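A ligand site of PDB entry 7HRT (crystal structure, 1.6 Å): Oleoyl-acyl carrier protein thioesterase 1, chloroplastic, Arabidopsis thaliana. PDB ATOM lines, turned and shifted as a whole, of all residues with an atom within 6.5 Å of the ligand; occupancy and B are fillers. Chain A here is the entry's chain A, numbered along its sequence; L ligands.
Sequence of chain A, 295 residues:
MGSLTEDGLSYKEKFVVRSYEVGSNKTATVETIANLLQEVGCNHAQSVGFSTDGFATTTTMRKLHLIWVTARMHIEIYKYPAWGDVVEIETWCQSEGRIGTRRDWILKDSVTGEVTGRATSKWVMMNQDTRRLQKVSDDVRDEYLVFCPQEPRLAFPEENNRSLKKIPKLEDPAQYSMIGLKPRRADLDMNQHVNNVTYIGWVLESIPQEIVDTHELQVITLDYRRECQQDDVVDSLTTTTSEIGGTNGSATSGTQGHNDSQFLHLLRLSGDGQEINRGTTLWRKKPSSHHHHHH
N of Ala 45 is in hydrogen-bond range of O1 of the ligand, 3.4 Å away.
O1 of the ligand sits at hydrogen-bond distance from ND1 of His 44, at 3.3 Å.
O of Ala 56 lies within hydrogen-bond range of O3 of the ligand (2.7 Å).
The guanidinium group of Arg 103 sits at hydrogen-bond distance from an oxygen (O1) of the ligand, at 3.2 Å.
The indole nitrogen of Trp 68 is in hydrogen-bond range of an oxygen (O3) of the ligand (2.8 Å).
Merely in contact with the ligand: Phe 50, Tyr 144, Cys 93, Phe 147 and Val 48.
Hydrophobic or aromatic side chains within 4 Å of the ligand: His 44, Val 48, Phe 50, Ala 56, Trp 68, Tyr 144 and Phe 147.
Ten residues have an atom within 4 Å of the ligand: His 44, Ala 45, Val 48, Phe 50, Ala 56, Trp 68, Cys 93, Arg 103, Tyr 144 and Phe 147.
The nearest printed residue that does not touch the ligand is Cys 148 (4.02 Å).
N of Trp 68 lies close to O of Phe 55 (3.4 Å).
The backbone carbonyl oxygen of His 44 sits at hydrogen-bond distance from the side-chain hydroxyl of Ser 47.
O of Tyr 144 lies within hydrogen-bond range of SG of Cys 148, at 3.6 Å.
NH1 of Arg 103 is in hydrogen-bond range of SG of Cys 93, at 2.8 Å.
The guanidinium group (NH2) of Arg 103 is in hydrogen-bond range of a ring nitrogen (ND1) of His 44 (2.8 Å).
NE1 of Trp 68 sits at hydrogen-bond distance from SD of Met 61, 3.7 Å away.
The backbone NH (N) of Phe 50 is in hydrogen-bond range of the backbone carbonyl oxygen (O) of Ala 45, 2.9 Å away.
The backbone carbonyl oxygen of Cys 93 sits close to the side-chain sulfur of Cys 148 (3.6 Å).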
ATOM      1  N   GLY A  41      21.125 -15.361 -12.638  1.00  0.00           N
ATOM      2  CA  GLY A  41      19.820 -15.074 -12.067  1.00  0.00           C
ATOM      3  C   GLY A  41      18.771 -16.069 -12.560  1.00  0.00           C
ATOM      4  O   GLY A  41      17.958 -16.545 -11.776  1.00  0.00           O
ATOM      5  N   ASN A  43      19.381 -19.166 -13.756  1.00  0.00           N
ATOM      6  CA  ASN A  43      19.696 -20.494 -13.224  1.00  0.00           C
ATOM      7  C   ASN A  43      19.285 -20.604 -11.747  1.00  0.00           C
ATOM      8  O   ASN A  43      18.748 -21.637 -11.370  1.00  0.00           O
ATOM      9  CB  ASN A  43      21.150 -20.907 -13.502  1.00  0.00           C
ATOM     10  CG  ASN A  43      21.389 -21.067 -14.993  1.00  0.00           C
ATOM     11  OD1 ASN A  43      20.461 -21.358 -15.783  1.00  0.00           O
ATOM     12  ND2 ASN A  43      22.626 -20.887 -15.432  1.00  0.00           N
ATOM     13  N   HIS A  44      19.388 -19.507 -10.982  1.00  0.00           N
ATOM     14  CA  HIS A  44      18.928 -19.495  -9.590  1.00  0.00           C
ATOM     15  C   HIS A  44      17.383 -19.678  -9.562  1.00  0.00           C
ATOM     16  O   HIS A  44      16.883 -20.566  -8.857  1.00  0.00           O
ATOM     17  CB  HIS A  44      19.327 -18.168  -8.913  1.00  0.00           C
ATOM     18  CG  HIS A  44      18.920 -18.043  -7.480  1.00  0.00           C
ATOM     19  ND1 HIS A  44      18.872 -16.816  -6.844  1.00  0.00           N
ATOM     20  CD2 HIS A  44      18.550 -19.010  -6.587  1.00  0.00           C
ATOM     21  CE1 HIS A  44      18.504 -17.066  -5.593  1.00  0.00           C
ATOM     22  NE2 HIS A  44      18.287 -18.373  -5.413  1.00  0.00           N
ATOM     23  N   ALA A  45      16.640 -18.906 -10.382  1.00  0.00           N
ATOM     24  CA  ALA A  45      15.171 -19.029 -10.430  1.00  0.00           C
ATOM     25  C   ALA A  45      14.736 -20.464 -10.801  1.00  0.00           C
ATOM     26  O   ALA A  45      13.853 -21.026 -10.150  1.00  0.00           O
ATOM     27  CB  ALA A  45      14.588 -18.028 -11.442  1.00  0.00           C
ATOM     28  N   GLN A  46      15.374 -21.069 -11.792  1.00  0.00           N
ATOM     29  CA  GLN A  46      15.048 -22.432 -12.226  1.00  0.00           C
ATOM     30  C   GLN A  46      15.299 -23.467 -11.110  1.00  0.00           C
ATOM     31  O   GLN A  46      14.489 -24.404 -10.945  1.00  0.00           O
ATOM     32  CB  GLN A  46      15.915 -22.790 -13.450  1.00  0.00           C
ATOM     33  CG  GLN A  46      15.651 -24.152 -14.072  1.00  0.00           C
ATOM     34  CD  GLN A  46      16.373 -24.264 -15.409  1.00  0.00           C
ATOM     35  OE1 GLN A  46      16.539 -23.268 -16.156  1.00  0.00           O
ATOM     36  NE2 GLN A  46      16.825 -25.477 -15.736  1.00  0.00           N
ATOM     37  N   SER A  47      16.406 -23.295 -10.372  1.00  0.00           N
ATOM     38  CA  SER A  47      16.799 -24.207  -9.306  1.00  0.00           C
ATOM     39  C   SER A  47      15.797 -24.264  -8.153  1.00  0.00           C
ATOM     40  O   SER A  47      15.687 -25.302  -7.510  1.00  0.00           O
ATOM     41  CB  SER A  47      18.182 -23.864  -8.779  1.00  0.00           C
ATOM     42  OG  SER A  47      18.170 -22.711  -7.946  1.00  0.00           O
ATOM     43  N   VAL A  48      15.072 -23.167  -7.886  1.00  0.00           N
ATOM     44  CA  VAL A  48      14.097 -23.161  -6.777  1.00  0.00           C
ATOM     45  C   VAL A  48      12.625 -23.193  -7.238  1.00  0.00           C
ATOM     46  O   VAL A  48      11.734 -22.954  -6.427  1.00  0.00           O
ATOM     47  CB  VAL A  48      14.350 -22.044  -5.747  1.00  0.00           C
ATOM     48  CG1 VAL A  48      15.744 -22.200  -5.121  1.00  0.00           C
ATOM     49  CG2 VAL A  48      14.183 -20.665  -6.368  1.00  0.00           C
ATOM     50  N   PHE A  50      10.988 -21.457 -10.058  1.00  0.00           N
ATOM     51  CA  PHE A  50      10.323 -20.282 -10.634  1.00  0.00           C
ATOM     52  C   PHE A  50      10.302 -20.310 -12.163  1.00  0.00           C
ATOM     53  O   PHE A  50      10.924 -21.185 -12.781  1.00  0.00           O
ATOM     54  CB  PHE A  50      10.931 -18.976 -10.106  1.00  0.00           C
ATOM     55  CG  PHE A  50      10.547 -18.685  -8.683  1.00  0.00           C
ATOM     56  CD1 PHE A  50       9.271 -18.276  -8.370  1.00  0.00           C
ATOM     57  CD2 PHE A  50      11.471 -18.799  -7.664  1.00  0.00           C
ATOM     58  CE1 PHE A  50       8.928 -18.008  -7.054  1.00  0.00           C
ATOM     59  CE2 PHE A  50      11.123 -18.519  -6.356  1.00  0.00           C
ATOM     60  CZ  PHE A  50       9.851 -18.121  -6.059  1.00  0.00           C
ATOM     61  N   PHE A  55      11.059 -13.237 -16.279  1.00  0.00           N
ATOM     62  CA  PHE A  55       9.996 -12.670 -15.433  1.00  0.00           C
ATOM     63  C   PHE A  55       9.876 -13.325 -14.032  1.00  0.00           C
ATOM     64  O   PHE A  55       9.152 -12.767 -13.213  1.00  0.00           O
ATOM     65  CB  PHE A  55       8.636 -12.690 -16.161  1.00  0.00           C
ATOM     66  CG  PHE A  55       8.636 -12.041 -17.529  1.00  0.00           C
ATOM     67  CD1 PHE A  55       9.056 -10.745 -17.712  1.00  0.00           C
ATOM     68  CD2 PHE A  55       8.120 -12.719 -18.626  1.00  0.00           C
ATOM     69  CE1 PHE A  55       9.021 -10.147 -18.963  1.00  0.00           C
ATOM     70  CE2 PHE A  55       8.086 -12.120 -19.878  1.00  0.00           C
ATOM     71  CZ  PHE A  55       8.541 -10.836 -20.044  1.00  0.00           C
ATOM     72  N   ALA A  56      10.565 -14.477 -13.774  1.00  0.00           N
ATOM     73  CA  ALA A  56      10.617 -15.213 -12.482  1.00  0.00           C
ATOM     74  C   ALA A  56       9.302 -15.246 -11.686  1.00  0.00           C
ATOM     75  O   ALA A  56       9.244 -14.867 -10.520  1.00  0.00           O
ATOM     76  CB  ALA A  56      11.753 -14.666 -11.615  1.00  0.00           C
ATOM     77  N   THR A  57       8.248 -15.699 -12.338  1.00  0.00           N
ATOM     78  CA  THR A  57       6.909 -15.725 -11.791  1.00  0.00           C
ATOM     79  C   THR A  57       6.570 -16.952 -10.949  1.00  0.00           C
ATOM     80  O   THR A  57       7.026 -18.066 -11.215  1.00  0.00           O
ATOM     81  CB  THR A  57       5.896 -15.574 -12.939  1.00  0.00           C
ATOM     82  OG1 THR A  57       5.967 -16.741 -13.760  1.00  0.00           O
ATOM     83  CG2 THR A  57       6.150 -14.344 -13.793  1.00  0.00           C
ATOM     84  N   THR A  58       5.728 -16.744  -9.939  1.00  0.00           N
ATOM     85  CA  THR A  58       5.150 -17.801  -9.081  1.00  0.00           C
ATOM     86  C   THR A  58       3.839 -18.277  -9.785  1.00  0.00           C
ATOM     87  O   THR A  58       3.337 -17.590 -10.695  1.00  0.00           O
ATOM     88  CB  THR A  58       4.806 -17.212  -7.683  1.00  0.00           C
ATOM     89  OG1 THR A  58       3.684 -16.331  -7.781  1.00  0.00           O
ATOM     90  CG2 THR A  58       5.969 -16.445  -7.049  1.00  0.00           C
ATOM     91  N   MET A  61       1.263 -15.466  -9.632  1.00  0.00           N
ATOM     92  CA  MET A  61       1.536 -14.374 -10.553  1.00  0.00           C
ATOM     93  C   MET A  61       1.066 -14.708 -11.964  1.00  0.00           C
ATOM     94  O   MET A  61       0.434 -13.873 -12.602  1.00  0.00           O
ATOM     95  CB  MET A  61       3.027 -14.003 -10.553  1.00  0.00           C
ATOM     96  CG  MET A  61       3.489 -13.329  -9.288  1.00  0.00           C
ATOM     97  SD  MET A  61       5.291 -13.048  -9.309  1.00  0.00           S
ATOM     98  CE  MET A  61       5.420 -11.855 -10.650  1.00  0.00           C
ATOM     99  N   TRP A  68       7.734  -9.721 -13.207  1.00  0.00           N
ATOM    100  CA  TRP A  68       8.746  -8.864 -12.605  1.00  0.00           C
ATOM    101  C   TRP A  68       9.461  -8.157 -13.767  1.00  0.00           C
ATOM    102  O   TRP A  68       9.775  -8.793 -14.774  1.00  0.00           O
ATOM    103  CB  TRP A  68       9.799  -9.701 -11.834  1.00  0.00           C
ATOM    104  CG  TRP A  68       9.323 -10.267 -10.517  1.00  0.00           C
ATOM    105  CD1 TRP A  68       9.144 -11.577 -10.194  1.00  0.00           C
ATOM    106  CD2 TRP A  68       9.005  -9.515  -9.342  1.00  0.00           C
ATOM    107  NE1 TRP A  68       8.729 -11.693  -8.892  1.00  0.00           N
ATOM    108  CE2 TRP A  68       8.612 -10.446  -8.346  1.00  0.00           C
ATOM    109  CE3 TRP A  68       8.997  -8.152  -9.029  1.00  0.00           C
ATOM    110  CZ2 TRP A  68       8.261 -10.042  -7.066  1.00  0.00           C
ATOM    111  CZ3 TRP A  68       8.634  -7.759  -7.757  1.00  0.00           C
ATOM    112  CH2 TRP A  68       8.276  -8.699  -6.794  1.00  0.00           C
ATOM    113  N   TRP A  92      21.633 -13.702  -5.053  1.00  0.00           N
ATOM    114  CA  TRP A  92      20.535 -13.950  -4.132  1.00  0.00           C
ATOM    115  C   TRP A  92      19.480 -12.857  -4.328  1.00  0.00           C
ATOM    116  O   TRP A  92      19.747 -11.794  -4.923  1.00  0.00           O
ATOM    117  CB  TRP A  92      21.046 -14.019  -2.671  1.00  0.00           C
ATOM    118  CG  TRP A  92      21.589 -12.701  -2.191  1.00  0.00           C
ATOM    119  CD1 TRP A  92      20.910 -11.725  -1.529  1.00  0.00           C
ATOM    120  CD2 TRP A  92      22.938 -12.225  -2.337  1.00  0.00           C
ATOM    121  NE1 TRP A  92      21.736 -10.648  -1.297  1.00  0.00           N
ATOM    122  CE2 TRP A  92      22.997 -10.939  -1.745  1.00  0.00           C
ATOM    123  CE3 TRP A  92      24.111 -12.766  -2.872  1.00  0.00           C
ATOM    124  CZ2 TRP A  92      24.180 -10.190  -1.704  1.00  0.00           C
ATOM    125  CZ3 TRP A  92      25.279 -12.017  -2.823  1.00  0.00           C
ATOM    126  CH2 TRP A  92      25.296 -10.742  -2.247  1.00  0.00           C
ATOM    127  N   CYS A  93      18.276 -13.119  -3.820  1.00  0.00           N
ATOM    128  CA  CYS A  93      17.167 -12.177  -3.903  1.00  0.00           C
ATOM    129  C   CYS A  93      16.751 -11.729  -2.523  1.00  0.00           C
ATOM    130  O   CYS A  93      16.890 -12.466  -1.555  1.00  0.00           O
ATOM    131  CB  CYS A  93      15.980 -12.806  -4.639  1.00  0.00           C
ATOM    132  SG  CYS A  93      16.278 -13.126  -6.377  1.00  0.00           S
ATOM    133  N   GLN A  94      16.173 -10.539  -2.442  1.00  0.00           N
ATOM    134  CA  GLN A  94      15.638 -10.041  -1.194  1.00  0.00           C
ATOM    135  C   GLN A  94      14.286  -9.416  -1.422  1.00  0.00           C
ATOM    136  O   GLN A  94      14.078  -8.736  -2.433  1.00  0.00           O
ATOM    137  CB  GLN A  94      16.587  -9.050  -0.533  1.00  0.00           C
ATOM    138  CG  GLN A  94      17.605  -9.768   0.348  1.00  0.00           C
ATOM    139  CD  GLN A  94      17.769  -9.075   1.681  1.00  0.00           C
ATOM    140  OE1 GLN A  94      18.383  -7.999   1.775  1.00  0.00           O
ATOM    141  NE2 GLN A  94      17.217  -9.692   2.723  1.00  0.00           N
ATOM    142  N   THR A 101      11.201  -6.413  -5.251  1.00  0.00           N
ATOM    143  CA  THR A 101      12.295  -7.287  -4.854  1.00  0.00           C
ATOM    144  C   THR A 101      13.623  -6.712  -5.364  1.00  0.00           C
ATOM    145  O   THR A 101      13.637  -5.847  -6.251  1.00  0.00           O
ATOM    146  CB  THR A 101      12.099  -8.742  -5.415  1.00  0.00           C
ATOM    147  OG1 THR A 101      11.839  -8.710  -6.826  1.00  0.00           O
ATOM    148  CG2 THR A 101      11.022  -9.525  -4.670  1.00  0.00           C
ATOM    149  N   ARG A 103      17.663  -8.127  -6.604  1.00  0.00           N
ATOM    150  CA  ARG A 103      18.567  -9.252  -6.833  1.00  0.00           C
ATOM    151  C   ARG A 103      19.938  -8.627  -6.765  1.00  0.00           C
ATOM    152  O   ARG A 103      20.191  -7.621  -7.472  1.00  0.00           O
ATOM    153  CB  ARG A 103      18.388  -9.944  -8.206  1.00  0.00           C
ATOM    154  CG  ARG A 103      19.442 -11.045  -8.447  1.00  0.00           C
ATOM    155  CD  ARG A 103      19.120 -11.913  -9.654  1.00  0.00           C
ATOM    156  NE  ARG A 103      17.960 -12.782  -9.451  1.00  0.00           N
ATOM    157  CZ  ARG A 103      18.002 -13.946  -8.801  1.00  0.00           C
ATOM    158  NH1 ARG A 103      16.913 -14.689  -8.667  1.00  0.00           N
ATOM    159  NH2 ARG A 103      19.136 -14.361  -8.240  1.00  0.00           N
ATOM    160  N   TYR A 144       7.017 -16.227  -1.887  1.00  0.00           N
ATOM    161  CA  TYR A 144       8.449 -16.283  -2.266  1.00  0.00           C
ATOM    162  C   TYR A 144       9.429 -15.921  -1.160  1.00  0.00           C
ATOM    163  O   TYR A 144      10.643 -15.990  -1.395  1.00  0.00           O
ATOM    164  CB  TYR A 144       8.735 -15.460  -3.512  1.00  0.00           C
ATOM    165  CG  TYR A 144       8.422 -13.982  -3.404  1.00  0.00           C
ATOM    166  CD1 TYR A 144       9.225 -13.122  -2.666  1.00  0.00           C
ATOM    167  CD2 TYR A 144       7.426 -13.414  -4.189  1.00  0.00           C
ATOM    168  CE1 TYR A 144       8.975 -11.761  -2.605  1.00  0.00           C
ATOM    169  CE2 TYR A 144       7.180 -12.044  -4.156  1.00  0.00           C
ATOM    170  CZ  TYR A 144       7.949 -11.213  -3.362  1.00  0.00           C
ATOM    171  OH  TYR A 144       7.696  -9.863  -3.329  1.00  0.00           O
ATOM    172  N   LEU A 145       8.948 -15.554   0.025  1.00  0.00           N
ATOM    173  CA  LEU A 145       9.828 -15.171   1.117  1.00  0.00           C
ATOM    174  C   LEU A 145      10.756 -16.296   1.575  1.00  0.00           C
ATOM    175  O   LEU A 145      11.885 -16.001   1.971  1.00  0.00           O
ATOM    176  CB  LEU A 145       9.037 -14.605   2.296  1.00  0.00           C
ATOM    177  CG  LEU A 145       8.952 -13.087   2.305  1.00  0.00           C
ATOM    178  CD1 LEU A 145       7.715 -12.599   3.071  1.00  0.00           C
ATOM    179  CD2 LEU A 145      10.248 -12.494   2.875  1.00  0.00           C
ATOM    180  N   PHE A 147      12.490 -18.299  -0.196  1.00  0.00           N
ATOM    181  CA  PHE A 147      13.613 -18.447  -1.099  1.00  0.00           C
ATOM    182  C   PHE A 147      14.668 -17.294  -0.891  1.00  0.00           C
ATOM    183  O   PHE A 147      15.678 -17.285  -1.559  1.00  0.00           O
ATOM    184  CB  PHE A 147      13.136 -18.520  -2.562  1.00  0.00           C
ATOM    185  CG  PHE A 147      12.127 -19.636  -2.745  1.00  0.00           C
ATOM    186  CD1 PHE A 147      12.522 -20.962  -2.671  1.00  0.00           C
ATOM    187  CD2 PHE A 147      10.784 -19.354  -2.884  1.00  0.00           C
ATOM    188  CE1 PHE A 147      11.581 -21.986  -2.761  1.00  0.00           C
ATOM    189  CE2 PHE A 147       9.844 -20.382  -3.007  1.00  0.00           C
ATOM    190  CZ  PHE A 147      10.249 -21.693  -2.917  1.00  0.00           C
ATOM    191  N   CYS A 148      14.393 -16.358   0.017  1.00  0.00           N
ATOM    192  CA  CYS A 148      15.265 -15.208   0.300  1.00  0.00           C
ATOM    193  C   CYS A 148      15.853 -15.275   1.695  1.00  0.00           C
ATOM    194  O   CYS A 148      15.141 -15.685   2.632  1.00  0.00           O
ATOM    195  CB  CYS A 148      14.444 -13.921   0.154  1.00  0.00           C
ATOM    196  SG  CYS A 148      13.545 -13.781  -1.412  1.00  0.00           S
HETATM  197  O1  LIG L   1      15.729 -17.373  -7.499  1.00  0.00           O
HETATM  198  C1  LIG L   1      14.904 -16.730  -6.877  1.00  0.00           C
HETATM  199  C2  LIG L   1      14.976 -16.394  -5.520  1.00  0.00           C
HETATM  200  C3  LIG L   1      13.994 -15.721  -4.908  1.00  0.00           C
HETATM  201  C4  LIG L   1      12.892 -15.211  -5.650  1.00  0.00           C
HETATM  202  O2  LIG L   1      13.784 -16.329  -7.581  1.00  0.00           O
HETATM  203  C5  LIG L   1      12.791 -15.573  -6.986  1.00  0.00           C
HETATM  204  C6  LIG L   1      11.712 -15.213  -7.787  1.00  0.00           C
HETATM  205  C7  LIG L   1      10.675 -14.499  -7.202  1.00  0.00           C
HETATM  206  O3  LIG L   1       9.564 -14.157  -7.892  1.00  0.00           O
HETATM  207  C8  LIG L   1      10.780 -14.073  -5.879  1.00  0.00           C
HETATM  208  C9  LIG L   1      11.826 -14.483  -5.092  1.00  0.00           C
